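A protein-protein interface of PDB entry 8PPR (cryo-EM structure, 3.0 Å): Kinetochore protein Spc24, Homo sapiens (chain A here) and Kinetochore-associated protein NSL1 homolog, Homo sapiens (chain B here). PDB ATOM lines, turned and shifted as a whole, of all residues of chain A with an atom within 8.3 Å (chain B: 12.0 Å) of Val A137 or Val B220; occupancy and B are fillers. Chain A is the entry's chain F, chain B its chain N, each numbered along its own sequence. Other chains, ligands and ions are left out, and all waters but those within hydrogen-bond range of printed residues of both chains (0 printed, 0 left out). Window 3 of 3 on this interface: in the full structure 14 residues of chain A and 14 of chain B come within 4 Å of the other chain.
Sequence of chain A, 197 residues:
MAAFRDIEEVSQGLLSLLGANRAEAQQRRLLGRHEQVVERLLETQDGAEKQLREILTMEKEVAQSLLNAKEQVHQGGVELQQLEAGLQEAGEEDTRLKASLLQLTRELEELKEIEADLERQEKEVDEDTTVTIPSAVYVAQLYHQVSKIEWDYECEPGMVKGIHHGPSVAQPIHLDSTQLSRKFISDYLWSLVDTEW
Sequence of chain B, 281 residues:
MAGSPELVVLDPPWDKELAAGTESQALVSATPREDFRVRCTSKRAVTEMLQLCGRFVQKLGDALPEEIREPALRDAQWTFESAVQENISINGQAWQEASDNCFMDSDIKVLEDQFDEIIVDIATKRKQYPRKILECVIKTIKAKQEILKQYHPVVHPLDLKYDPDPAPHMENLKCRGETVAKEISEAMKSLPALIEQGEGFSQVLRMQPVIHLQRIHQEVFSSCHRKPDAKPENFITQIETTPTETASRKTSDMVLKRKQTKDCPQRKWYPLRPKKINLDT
N of Tyr A153 is in hydrogen-bond range of OE1 of Gln B214, 2.5 Å away. O of Val B220 is in hydrogen-bond range of NE2 of Gln A141 (3.2 Å).
The backbone carbonyl oxygen (O) of Glu B219 is in hydrogen-bond range of the side-chain hydroxyl (OG) of Ser B222 (3.0 Å).
Among the printed residues, pairs that only touch across the chains: His A144 with Phe B221 (3.4 Å), Gln A141 with Ser B222 (3.6 Å), Tyr A153 with His B217 (3.6 Å), Ala A140 with Val B220 (3.7 Å), Tyr A153 with Ile B216 (3.7 Å), Trp A151 with Gln B214 (3.8 Å), Trp A151 with Ile B211 (3.8 Å) and Val A137 with Val B220 (3.97 Å).
Of the printed residues of chain B, Val A137 touches Val B220. Val B220 touches just these residues of chain A: Val A137, Ala A140 and Gln A141. No residue of chain B comes within 4 Å of Pro A134. No residue of chain B comes within 4 Å of Ser A135. No residue of chain B comes within 4 Å of Ala A136. No residue of chain B comes within 4 Å of Tyr A138. No residue of chain B comes within 4 Å of Val A139. Ala A140 touches one residue of chain B. Gln A141 touches just these residues of chain B: Val B220 (3.2 Å) and Ser B222 (3.6 Å). Printed residues of chain A within 4 Å of Ser B222: Gln A141. Of the printed residues of chain B, His A144 touches Phe B221 (3.4 Å). Of the printed residues of chain A, Ile B211 touches Trp A151 (3.8 Å). His B212 touches none of the printed residues of chain A.
Printed residues of chain A that touch a printed residue of chain B: Val A137, Ala A140, Gln A141, His A144, Trp A151 and Tyr A153. Printed residues of chain B that touch a printed residue of chain A: Ile B211, Gln B214, Ile B216, His B217, Val B220, Phe B221 and Ser B222. Along chain B the printed residues that touch a printed residue of chain A span positions 211 to 222. Among the printed residues, no Asp or Glu carboxylate lies within 4 Å of a Lys or Arg side-chain nitrogen of the other chain.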
ATOM      1  N   THR A 129      18.870   0.876  14.738  1.00  0.00           N
ATOM      2  CA  THR A 129      19.373  -0.387  14.205  1.00  0.00           C
ATOM      3  C   THR A 129      18.320  -1.129  13.392  1.00  0.00           C
ATOM      4  O   THR A 129      18.594  -1.565  12.265  1.00  0.00           O
ATOM      5  CB  THR A 129      19.870  -1.281  15.343  1.00  0.00           C
ATOM      6  OG1 THR A 129      20.675  -0.510  16.242  1.00  0.00           O
ATOM      7  CG2 THR A 129      20.690  -2.437  14.794  1.00  0.00           C
ATOM      8  N   VAL A 131      15.588   0.069  11.899  1.00  0.00           N
ATOM      9  CA  VAL A 131      15.336   0.764  10.640  1.00  0.00           C
ATOM     10  C   VAL A 131      16.487   0.525   9.669  1.00  0.00           C
ATOM     11  O   VAL A 131      16.287  -0.018   8.578  1.00  0.00           O
ATOM     12  CB  VAL A 131      15.110   2.269  10.862  1.00  0.00           C
ATOM     13  CG1 VAL A 131      15.020   2.985   9.526  1.00  0.00           C
ATOM     14  CG2 VAL A 131      13.837   2.488  11.651  1.00  0.00           C
ATOM     15  N   THR A 132      17.693   0.917  10.073  1.00  0.00           N
ATOM     16  CA  THR A 132      18.889   0.854   9.242  1.00  0.00           C
ATOM     17  C   THR A 132      19.096  -0.499   8.580  1.00  0.00           C
ATOM     18  O   THR A 132      19.115  -0.587   7.348  1.00  0.00           O
ATOM     19  CB  THR A 132      20.134   1.196  10.066  1.00  0.00           C
ATOM     20  OG1 THR A 132      20.365   0.168  11.039  1.00  0.00           O
ATOM     21  CG2 THR A 132      19.976   2.539  10.756  1.00  0.00           C
ATOM     22  N   ILE A 133      19.253  -1.554   9.374  1.00  0.00           N
ATOM     23  CA  ILE A 133      19.789  -2.800   8.831  1.00  0.00           C
ATOM     24  C   ILE A 133      18.801  -3.444   7.856  1.00  0.00           C
ATOM     25  O   ILE A 133      19.177  -3.652   6.693  1.00  0.00           O
ATOM     26  CB  ILE A 133      20.236  -3.753   9.954  1.00  0.00           C
ATOM     27  CG1 ILE A 133      21.172  -3.022  10.917  1.00  0.00           C
ATOM     28  CG2 ILE A 133      20.899  -4.989   9.370  1.00  0.00           C
ATOM     29  CD1 ILE A 133      22.376  -2.407  10.238  1.00  0.00           C
ATOM     30  N   PRO A 134      17.542  -3.799   8.247  1.00  0.00           N
ATOM     31  CA  PRO A 134      16.573  -4.215   7.224  1.00  0.00           C
ATOM     32  C   PRO A 134      16.519  -3.302   6.010  1.00  0.00           C
ATOM     33  O   PRO A 134      16.568  -3.782   4.876  1.00  0.00           O
ATOM     34  CB  PRO A 134      15.244  -4.190   7.984  1.00  0.00           C
ATOM     35  CG  PRO A 134      15.611  -4.500   9.395  1.00  0.00           C
ATOM     36  CD  PRO A 134      17.111  -4.333   9.553  1.00  0.00           C
ATOM     37  N   SER A 135      16.436  -1.989   6.225  1.00  0.00           N
ATOM     38  CA  SER A 135      16.272  -1.079   5.096  1.00  0.00           C
ATOM     39  C   SER A 135      17.498  -1.091   4.191  1.00  0.00           C
ATOM     40  O   SER A 135      17.392  -1.384   2.999  1.00  0.00           O
ATOM     41  CB  SER A 135      15.988   0.340   5.589  1.00  0.00           C
ATOM     42  OG  SER A 135      15.922   1.248   4.502  1.00  0.00           O
ATOM     43  N   ALA A 136      18.667  -0.769   4.744  1.00  0.00           N
ATOM     44  CA  ALA A 136      19.864  -0.624   3.921  1.00  0.00           C
ATOM     45  C   ALA A 136      20.271  -1.950   3.288  1.00  0.00           C
ATOM     46  O   ALA A 136      20.576  -2.014   2.090  1.00  0.00           O
ATOM     47  CB  ALA A 136      21.003  -0.046   4.759  1.00  0.00           C
ATOM     48  N   VAL A 137      20.294  -3.024   4.085  1.00  0.00           N
ATOM     49  CA  VAL A 137      20.714  -4.325   3.566  1.00  0.00           C
ATOM     50  C   VAL A 137      19.797  -4.773   2.439  1.00  0.00           C
ATOM     51  O   VAL A 137      20.259  -5.199   1.374  1.00  0.00           O
ATOM     52  CB  VAL A 137      20.760  -5.366   4.701  1.00  0.00           C
ATOM     53  CG1 VAL A 137      20.933  -6.763   4.130  1.00  0.00           C
ATOM     54  CG2 VAL A 137      21.888  -5.048   5.664  1.00  0.00           C
ATOM     55  N   TYR A 138      18.487  -4.667   2.644  1.00  0.00           N
ATOM     56  CA  TYR A 138      17.544  -5.115   1.629  1.00  0.00           C
ATOM     57  C   TYR A 138      17.520  -4.204   0.413  1.00  0.00           C
ATOM     58  O   TYR A 138      17.341  -4.695  -0.705  1.00  0.00           O
ATOM     59  CB  TYR A 138      16.141  -5.236   2.226  1.00  0.00           C
ATOM     60  CG  TYR A 138      16.016  -6.400   3.182  1.00  0.00           C
ATOM     61  CD1 TYR A 138      16.786  -7.543   3.013  1.00  0.00           C
ATOM     62  CD2 TYR A 138      15.146  -6.353   4.262  1.00  0.00           C
ATOM     63  CE1 TYR A 138      16.684  -8.610   3.884  1.00  0.00           C
ATOM     64  CE2 TYR A 138      15.042  -7.411   5.144  1.00  0.00           C
ATOM     65  CZ  TYR A 138      15.809  -8.539   4.946  1.00  0.00           C
ATOM     66  OH  TYR A 138      15.706  -9.599   5.817  1.00  0.00           O
ATOM     67  N   VAL A 139      17.721  -2.898   0.591  1.00  0.00           N
ATOM     68  CA  VAL A 139      17.833  -1.999  -0.553  1.00  0.00           C
ATOM     69  C   VAL A 139      19.049  -2.363  -1.394  1.00  0.00           C
ATOM     70  O   VAL A 139      18.974  -2.431  -2.625  1.00  0.00           O
ATOM     71  CB  VAL A 139      17.891  -0.536  -0.084  1.00  0.00           C
ATOM     72  CG1 VAL A 139      18.487   0.348  -1.168  1.00  0.00           C
ATOM     73  CG2 VAL A 139      16.505  -0.045   0.285  1.00  0.00           C
ATOM     74  N   ALA A 140      20.188  -2.601  -0.741  1.00  0.00           N
ATOM     75  CA  ALA A 140      21.390  -2.976  -1.477  1.00  0.00           C
ATOM     76  C   ALA A 140      21.210  -4.312  -2.184  1.00  0.00           C
ATOM     77  O   ALA A 140      21.615  -4.468  -3.343  1.00  0.00           O
ATOM     78  CB  ALA A 140      22.588  -3.021  -0.532  1.00  0.00           C
ATOM     79  N   GLN A 141      20.599  -5.286  -1.507  1.00  0.00           N
ATOM     80  CA  GLN A 141      20.388  -6.589  -2.126  1.00  0.00           C
ATOM     81  C   GLN A 141      19.415  -6.496  -3.293  1.00  0.00           C
ATOM     82  O   GLN A 141      19.589  -7.183  -4.304  1.00  0.00           O
ATOM     83  CB  GLN A 141      19.901  -7.595  -1.085  1.00  0.00           C
ATOM     84  CG  GLN A 141      20.952  -7.944  -0.044  1.00  0.00           C
ATOM     85  CD  GLN A 141      20.608  -9.190   0.745  1.00  0.00           C
ATOM     86  OE1 GLN A 141      19.502  -9.720   0.639  1.00  0.00           O
ATOM     87  NE2 GLN A 141      21.559  -9.670   1.539  1.00  0.00           N
ATOM     88  N   LEU A 142      18.387  -5.654  -3.177  1.00  0.00           N
ATOM     89  CA  LEU A 142      17.467  -5.456  -4.288  1.00  0.00           C
ATOM     90  C   LEU A 142      18.158  -4.768  -5.459  1.00  0.00           C
ATOM     91  O   LEU A 142      17.943  -5.140  -6.619  1.00  0.00           O
ATOM     92  CB  LEU A 142      16.256  -4.653  -3.818  1.00  0.00           C
ATOM     93  CG  LEU A 142      15.293  -4.169  -4.900  1.00  0.00           C
ATOM     94  CD1 LEU A 142      14.445  -5.325  -5.402  1.00  0.00           C
ATOM     95  CD2 LEU A 142      14.418  -3.048  -4.368  1.00  0.00           C
ATOM     96  N   TYR A 143      18.997  -3.767  -5.172  1.00  0.00           N
ATOM     97  CA  TYR A 143      19.816  -3.149  -6.211  1.00  0.00           C
ATOM     98  C   TYR A 143      20.642  -4.197  -6.941  1.00  0.00           C
ATOM     99  O   TYR A 143      20.675  -4.237  -8.176  1.00  0.00           O
ATOM    100  CB  TYR A 143      20.743  -2.100  -5.595  1.00  0.00           C
ATOM    101  CG  TYR A 143      20.231  -0.679  -5.609  1.00  0.00           C
ATOM    102  CD1 TYR A 143      19.897  -0.049  -6.799  1.00  0.00           C
ATOM    103  CD2 TYR A 143      20.116   0.046  -4.429  1.00  0.00           C
ATOM    104  CE1 TYR A 143      19.442   1.257  -6.813  1.00  0.00           C
ATOM    105  CE2 TYR A 143      19.662   1.350  -4.433  1.00  0.00           C
ATOM    106  CZ  TYR A 143      19.326   1.951  -5.627  1.00  0.00           C
ATOM    107  OH  TYR A 143      18.873   3.250  -5.638  1.00  0.00           O
ATOM    108  N   HIS A 144      21.319  -5.056  -6.181  1.00  0.00           N
ATOM    109  CA  HIS A 144      22.204  -6.043  -6.787  1.00  0.00           C
ATOM    110  C   HIS A 144      21.417  -7.075  -7.583  1.00  0.00           C
ATOM    111  O   HIS A 144      21.836  -7.480  -8.671  1.00  0.00           O
ATOM    112  CB  HIS A 144      23.046  -6.717  -5.707  1.00  0.00           C
ATOM    113  CG  HIS A 144      23.783  -7.925  -6.186  1.00  0.00           C
ATOM    114  ND1 HIS A 144      23.276  -9.200  -6.070  1.00  0.00           N
ATOM    115  CD2 HIS A 144      24.986  -8.051  -6.793  1.00  0.00           C
ATOM    116  CE1 HIS A 144      24.141 -10.059  -6.577  1.00  0.00           C
ATOM    117  NE2 HIS A 144      25.185  -9.388  -7.026  1.00  0.00           N
ATOM    118  N   ILE A 149      25.161  -7.026 -10.515  1.00  0.00           N
ATOM    119  CA  ILE A 149      26.466  -6.387 -10.579  1.00  0.00           C
ATOM    120  C   ILE A 149      27.063  -6.340  -9.182  1.00  0.00           C
ATOM    121  O   ILE A 149      26.415  -5.881  -8.236  1.00  0.00           O
ATOM    122  CB  ILE A 149      26.368  -4.967 -11.172  1.00  0.00           C
ATOM    123  CG1 ILE A 149      25.869  -5.026 -12.616  1.00  0.00           C
ATOM    124  CG2 ILE A 149      27.699  -4.243 -11.050  1.00  0.00           C
ATOM    125  CD1 ILE A 149      25.856  -3.688 -13.316  1.00  0.00           C
ATOM    126  N   TRP A 151      30.248  -4.801  -7.087  1.00  0.00           N
ATOM    127  CA  TRP A 151      31.255  -3.758  -7.192  1.00  0.00           C
ATOM    128  C   TRP A 151      32.541  -4.154  -6.480  1.00  0.00           C
ATOM    129  O   TRP A 151      32.550  -4.971  -5.558  1.00  0.00           O
ATOM    130  CB  TRP A 151      30.735  -2.442  -6.616  1.00  0.00           C
ATOM    131  CG  TRP A 151      29.444  -2.007  -7.207  1.00  0.00           C
ATOM    132  CD1 TRP A 151      28.229  -1.968  -6.591  1.00  0.00           C
ATOM    133  CD2 TRP A 151      29.233  -1.542  -8.542  1.00  0.00           C
ATOM    134  NE1 TRP A 151      27.272  -1.506  -7.461  1.00  0.00           N
ATOM    135  CE2 TRP A 151      27.864  -1.239  -8.667  1.00  0.00           C
ATOM    136  CE3 TRP A 151      30.070  -1.353  -9.645  1.00  0.00           C
ATOM    137  CZ2 TRP A 151      27.314  -0.756  -9.850  1.00  0.00           C
ATOM    138  CZ3 TRP A 151      29.523  -0.876 -10.816  1.00  0.00           C
ATOM    139  CH2 TRP A 151      28.157  -0.584 -10.911  1.00  0.00           C
ATOM    140  N   TYR A 153      34.726  -2.464  -4.143  1.00  0.00           N
ATOM    141  CA  TYR A 153      34.649  -1.271  -3.310  1.00  0.00           C
ATOM    142  C   TYR A 153      36.025  -0.738  -2.941  1.00  0.00           C
ATOM    143  O   TYR A 153      36.179   0.470  -2.731  1.00  0.00           O
ATOM    144  CB  TYR A 153      33.847  -1.573  -2.045  1.00  0.00           C
ATOM    145  CG  TYR A 153      32.459  -2.087  -2.340  1.00  0.00           C
ATOM    146  CD1 TYR A 153      31.490  -1.254  -2.879  1.00  0.00           C
ATOM    147  CD2 TYR A 153      32.120  -3.409  -2.086  1.00  0.00           C
ATOM    148  CE1 TYR A 153      30.222  -1.723  -3.156  1.00  0.00           C
ATOM    149  CE2 TYR A 153      30.856  -3.887  -2.358  1.00  0.00           C
ATOM    150  CZ  TYR A 153      29.911  -3.041  -2.892  1.00  0.00           C
ATOM    151  OH  TYR A 153      28.648  -3.512  -3.165  1.00  0.00           O
ATOM    152  N   ILE B 211      36.970  -9.704  -4.230  1.00  0.00           N
ATOM    153  CA  ILE B 211      35.737  -8.943  -4.069  1.00  0.00           C
ATOM    154  C   ILE B 211      34.918  -9.509  -2.919  1.00  0.00           C
ATOM    155  O   ILE B 211      34.350  -8.760  -2.112  1.00  0.00           O
ATOM    156  CB  ILE B 211      34.942  -8.923  -5.386  1.00  0.00           C
ATOM    157  CG1 ILE B 211      35.535  -7.890  -6.345  1.00  0.00           C
ATOM    158  CG2 ILE B 211      33.474  -8.621  -5.126  1.00  0.00           C
ATOM    159  CD1 ILE B 211      34.818  -7.809  -7.675  1.00  0.00           C
ATOM    160  N   HIS B 212      34.855 -10.839  -2.810  1.00  0.00           N
ATOM    161  CA  HIS B 212      34.136 -11.455  -1.702  1.00  0.00           C
ATOM    162  C   HIS B 212      34.773 -11.152  -0.352  1.00  0.00           C
ATOM    163  O   HIS B 212      34.093 -11.248   0.674  1.00  0.00           O
ATOM    164  CB  HIS B 212      34.052 -12.966  -1.907  1.00  0.00           C
ATOM    165  CG  HIS B 212      32.850 -13.398  -2.687  1.00  0.00           C
ATOM    166  ND1 HIS B 212      32.255 -14.630  -2.516  1.00  0.00           N
ATOM    167  CD2 HIS B 212      32.122 -12.756  -3.629  1.00  0.00           C
ATOM    168  CE1 HIS B 212      31.218 -14.731  -3.328  1.00  0.00           C
ATOM    169  NE2 HIS B 212      31.116 -13.607  -4.015  1.00  0.00           N
ATOM    170  N   LEU B 213      36.054 -10.788  -0.329  1.00  0.00           N
ATOM    171  CA  LEU B 213      36.728 -10.475   0.923  1.00  0.00           C
ATOM    172  C   LEU B 213      36.499  -9.040   1.380  1.00  0.00           C
ATOM    173  O   LEU B 213      36.886  -8.699   2.502  1.00  0.00           O
ATOM    174  CB  LEU B 213      38.230 -10.733   0.789  1.00  0.00           C
ATOM    175  CG  LEU B 213      38.655 -12.193   0.614  1.00  0.00           C
ATOM    176  CD1 LEU B 213      40.100 -12.383   1.040  1.00  0.00           C
ATOM    177  CD2 LEU B 213      37.734 -13.126   1.388  1.00  0.00           C
ATOM    178  N   GLN B 214      35.888  -8.203   0.549  1.00  0.00           N
ATOM    179  CA  GLN B 214      35.683  -6.808   0.910  1.00  0.00           C
ATOM    180  C   GLN B 214      34.653  -6.689   2.027  1.00  0.00           C
ATOM    181  O   GLN B 214      33.616  -7.357   2.011  1.00  0.00           O
ATOM    182  CB  GLN B 214      35.237  -6.013  -0.315  1.00  0.00           C
ATOM    183  CG  GLN B 214      36.197  -6.137  -1.485  1.00  0.00           C
ATOM    184  CD  GLN B 214      35.967  -5.085  -2.548  1.00  0.00           C
ATOM    185  OE1 GLN B 214      34.888  -4.509  -2.641  1.00  0.00           O
ATOM    186  NE2 GLN B 214      36.988  -4.829  -3.356  1.00  0.00           N
ATOM    187  N   ARG B 215      34.949  -5.826   3.002  1.00  0.00           N
ATOM    188  CA  ARG B 215      34.073  -5.683   4.160  1.00  0.00           C
ATOM    189  C   ARG B 215      32.698  -5.165   3.762  1.00  0.00           C
ATOM    190  O   ARG B 215      31.679  -5.631   4.283  1.00  0.00           O
ATOM    191  CB  ARG B 215      34.707  -4.752   5.189  1.00  0.00           C
ATOM    192  CG  ARG B 215      33.961  -4.712   6.509  1.00  0.00           C
ATOM    193  CD  ARG B 215      34.300  -5.919   7.365  1.00  0.00           C
ATOM    194  NE  ARG B 215      35.730  -6.209   7.359  1.00  0.00           N
ATOM    195  CZ  ARG B 215      36.654  -5.456   7.941  1.00  0.00           C
ATOM    196  NH1 ARG B 215      36.334  -4.362   8.614  1.00  0.00           N
ATOM    197  NH2 ARG B 215      37.933  -5.813   7.851  1.00  0.00           N
ATOM    198  N   ILE B 216      32.652  -4.188   2.854  1.00  0.00           N
ATOM    199  CA  ILE B 216      31.370  -3.659   2.401  1.00  0.00           C
ATOM    200  C   ILE B 216      30.559  -4.754   1.727  1.00  0.00           C
ATOM    201  O   ILE B 216      29.360  -4.911   1.986  1.00  0.00           O
ATOM    202  CB  ILE B 216      31.593  -2.460   1.464  1.00  0.00           C
ATOM    203  CG1 ILE B 216      32.442  -1.397   2.159  1.00  0.00           C
ATOM    204  CG2 ILE B 216      30.262  -1.882   1.017  1.00  0.00           C
ATOM    205  CD1 ILE B 216      32.629  -0.139   1.344  1.00  0.00           C
ATOM    206  N   HIS B 217      31.206  -5.535   0.861  1.00  0.00           N
ATOM    207  CA  HIS B 217      30.526  -6.649   0.211  1.00  0.00           C
ATOM    208  C   HIS B 217      30.039  -7.665   1.234  1.00  0.00           C
ATOM    209  O   HIS B 217      28.921  -8.182   1.126  1.00  0.00           O
ATOM    210  CB  HIS B 217      31.465  -7.306  -0.800  1.00  0.00           C
ATOM    211  CG  HIS B 217      30.910  -8.544  -1.430  1.00  0.00           C
ATOM    212  ND1 HIS B 217      30.901  -9.766  -0.790  1.00  0.00           N
ATOM    213  CD2 HIS B 217      30.352  -8.753  -2.645  1.00  0.00           C
ATOM    214  CE1 HIS B 217      30.356 -10.671  -1.582  1.00  0.00           C
ATOM    215  NE2 HIS B 217      30.014 -10.083  -2.714  1.00  0.00           N
ATOM    216  N   GLN B 218      30.869  -7.963   2.237  1.00  0.00           N
ATOM    217  CA  GLN B 218      30.483  -8.932   3.256  1.00  0.00           C
ATOM    218  C   GLN B 218      29.262  -8.459   4.032  1.00  0.00           C
ATOM    219  O   GLN B 218      28.328  -9.234   4.270  1.00  0.00           O
ATOM    220  CB  GLN B 218      31.656  -9.177   4.201  1.00  0.00           C
ATOM    221  CG  GLN B 218      32.785  -9.976   3.582  1.00  0.00           C
ATOM    222  CD  GLN B 218      33.741 -10.522   4.618  1.00  0.00           C
ATOM    223  OE1 GLN B 218      33.394 -10.653   5.792  1.00  0.00           O
ATOM    224  NE2 GLN B 218      34.956 -10.840   4.191  1.00  0.00           N
ATOM    225  N   GLU B 219      29.252  -7.187   4.433  1.00  0.00           N
ATOM    226  CA  GLU B 219      28.116  -6.656   5.176  1.00  0.00           C
ATOM    227  C   GLU B 219      26.860  -6.629   4.316  1.00  0.00           C
ATOM    228  O   GLU B 219      25.770  -6.975   4.787  1.00  0.00           O
ATOM    229  CB  GLU B 219      28.438  -5.256   5.692  1.00  0.00           C
ATOM    230  CG  GLU B 219      29.452  -5.231   6.820  1.00  0.00           C
ATOM    231  CD  GLU B 219      29.750  -3.826   7.297  1.00  0.00           C
ATOM    232  OE1 GLU B 219      29.029  -2.894   6.884  1.00  0.00           O
ATOM    233  OE2 GLU B 219      30.704  -3.651   8.083  1.00  0.00           O
ATOM    234  N   VAL B 220      26.993  -6.222   3.054  1.00  0.00           N
ATOM    235  CA  VAL B 220      25.839  -6.180   2.163  1.00  0.00           C
ATOM    236  C   VAL B 220      25.305  -7.582   1.911  1.00  0.00           C
ATOM    237  O   VAL B 220      24.093  -7.819   1.967  1.00  0.00           O
ATOM    238  CB  VAL B 220      26.210  -5.471   0.849  1.00  0.00           C
ATOM    239  CG1 VAL B 220      25.111  -5.662  -0.181  1.00  0.00           C
ATOM    240  CG2 VAL B 220      26.453  -3.994   1.098  1.00  0.00           C
ATOM    241  N   PHE B 221      26.196  -8.536   1.647  1.00  0.00           N
ATOM    242  CA  PHE B 221      25.803  -9.889   1.286  1.00  0.00           C
ATOM    243  C   PHE B 221      25.764 -10.824   2.486  1.00  0.00           C
ATOM    244  O   PHE B 221      25.873 -12.042   2.319  1.00  0.00           O
ATOM    245  CB  PHE B 221      26.741 -10.436   0.213  1.00  0.00           C
ATOM    246  CG  PHE B 221      26.531  -9.818  -1.136  1.00  0.00           C
ATOM    247  CD1 PHE B 221      25.613 -10.351  -2.021  1.00  0.00           C
ATOM    248  CD2 PHE B 221      27.239  -8.690  -1.510  1.00  0.00           C
ATOM    249  CE1 PHE B 221      25.412  -9.780  -3.262  1.00  0.00           C
ATOM    250  CE2 PHE B 221      27.043  -8.113  -2.750  1.00  0.00           C
ATOM    251  CZ  PHE B 221      26.128  -8.658  -3.627  1.00  0.00           C
ATOM    252  N   SER B 222      25.614 -10.278   3.690  1.00  0.00           N
ATOM    253  CA  SER B 222      25.428 -11.119   4.862  1.00  0.00           C
ATOM    254  C   SER B 222      24.113 -11.879   4.754  1.00  0.00           C
ATOM    255  O   SER B 222      23.083 -11.322   4.367  1.00  0.00           O
ATOM    256  CB  SER B 222      25.448 -10.267   6.131  1.00  0.00           C
ATOM    257  OG  SER B 222      24.428  -9.285   6.096  1.00  0.00           O
ATOM    258  N   SER B 223      24.155 -13.164   5.095  1.00  0.00           N
ATOM    259  CA  SER B 223      22.980 -14.020   4.987  1.00  0.00           C
ATOM    260  C   SER B 223      21.905 -13.615   5.989  1.00  0.00           C
ATOM    261  O   SER B 223      20.878 -13.049   5.616  1.00  0.00           O
ATOM    262  CB  SER B 223      23.364 -15.487   5.194  1.00  0.00           C
ATOM    263  OG  SER B 223      22.241 -16.335   5.034  1.00  0.00           O
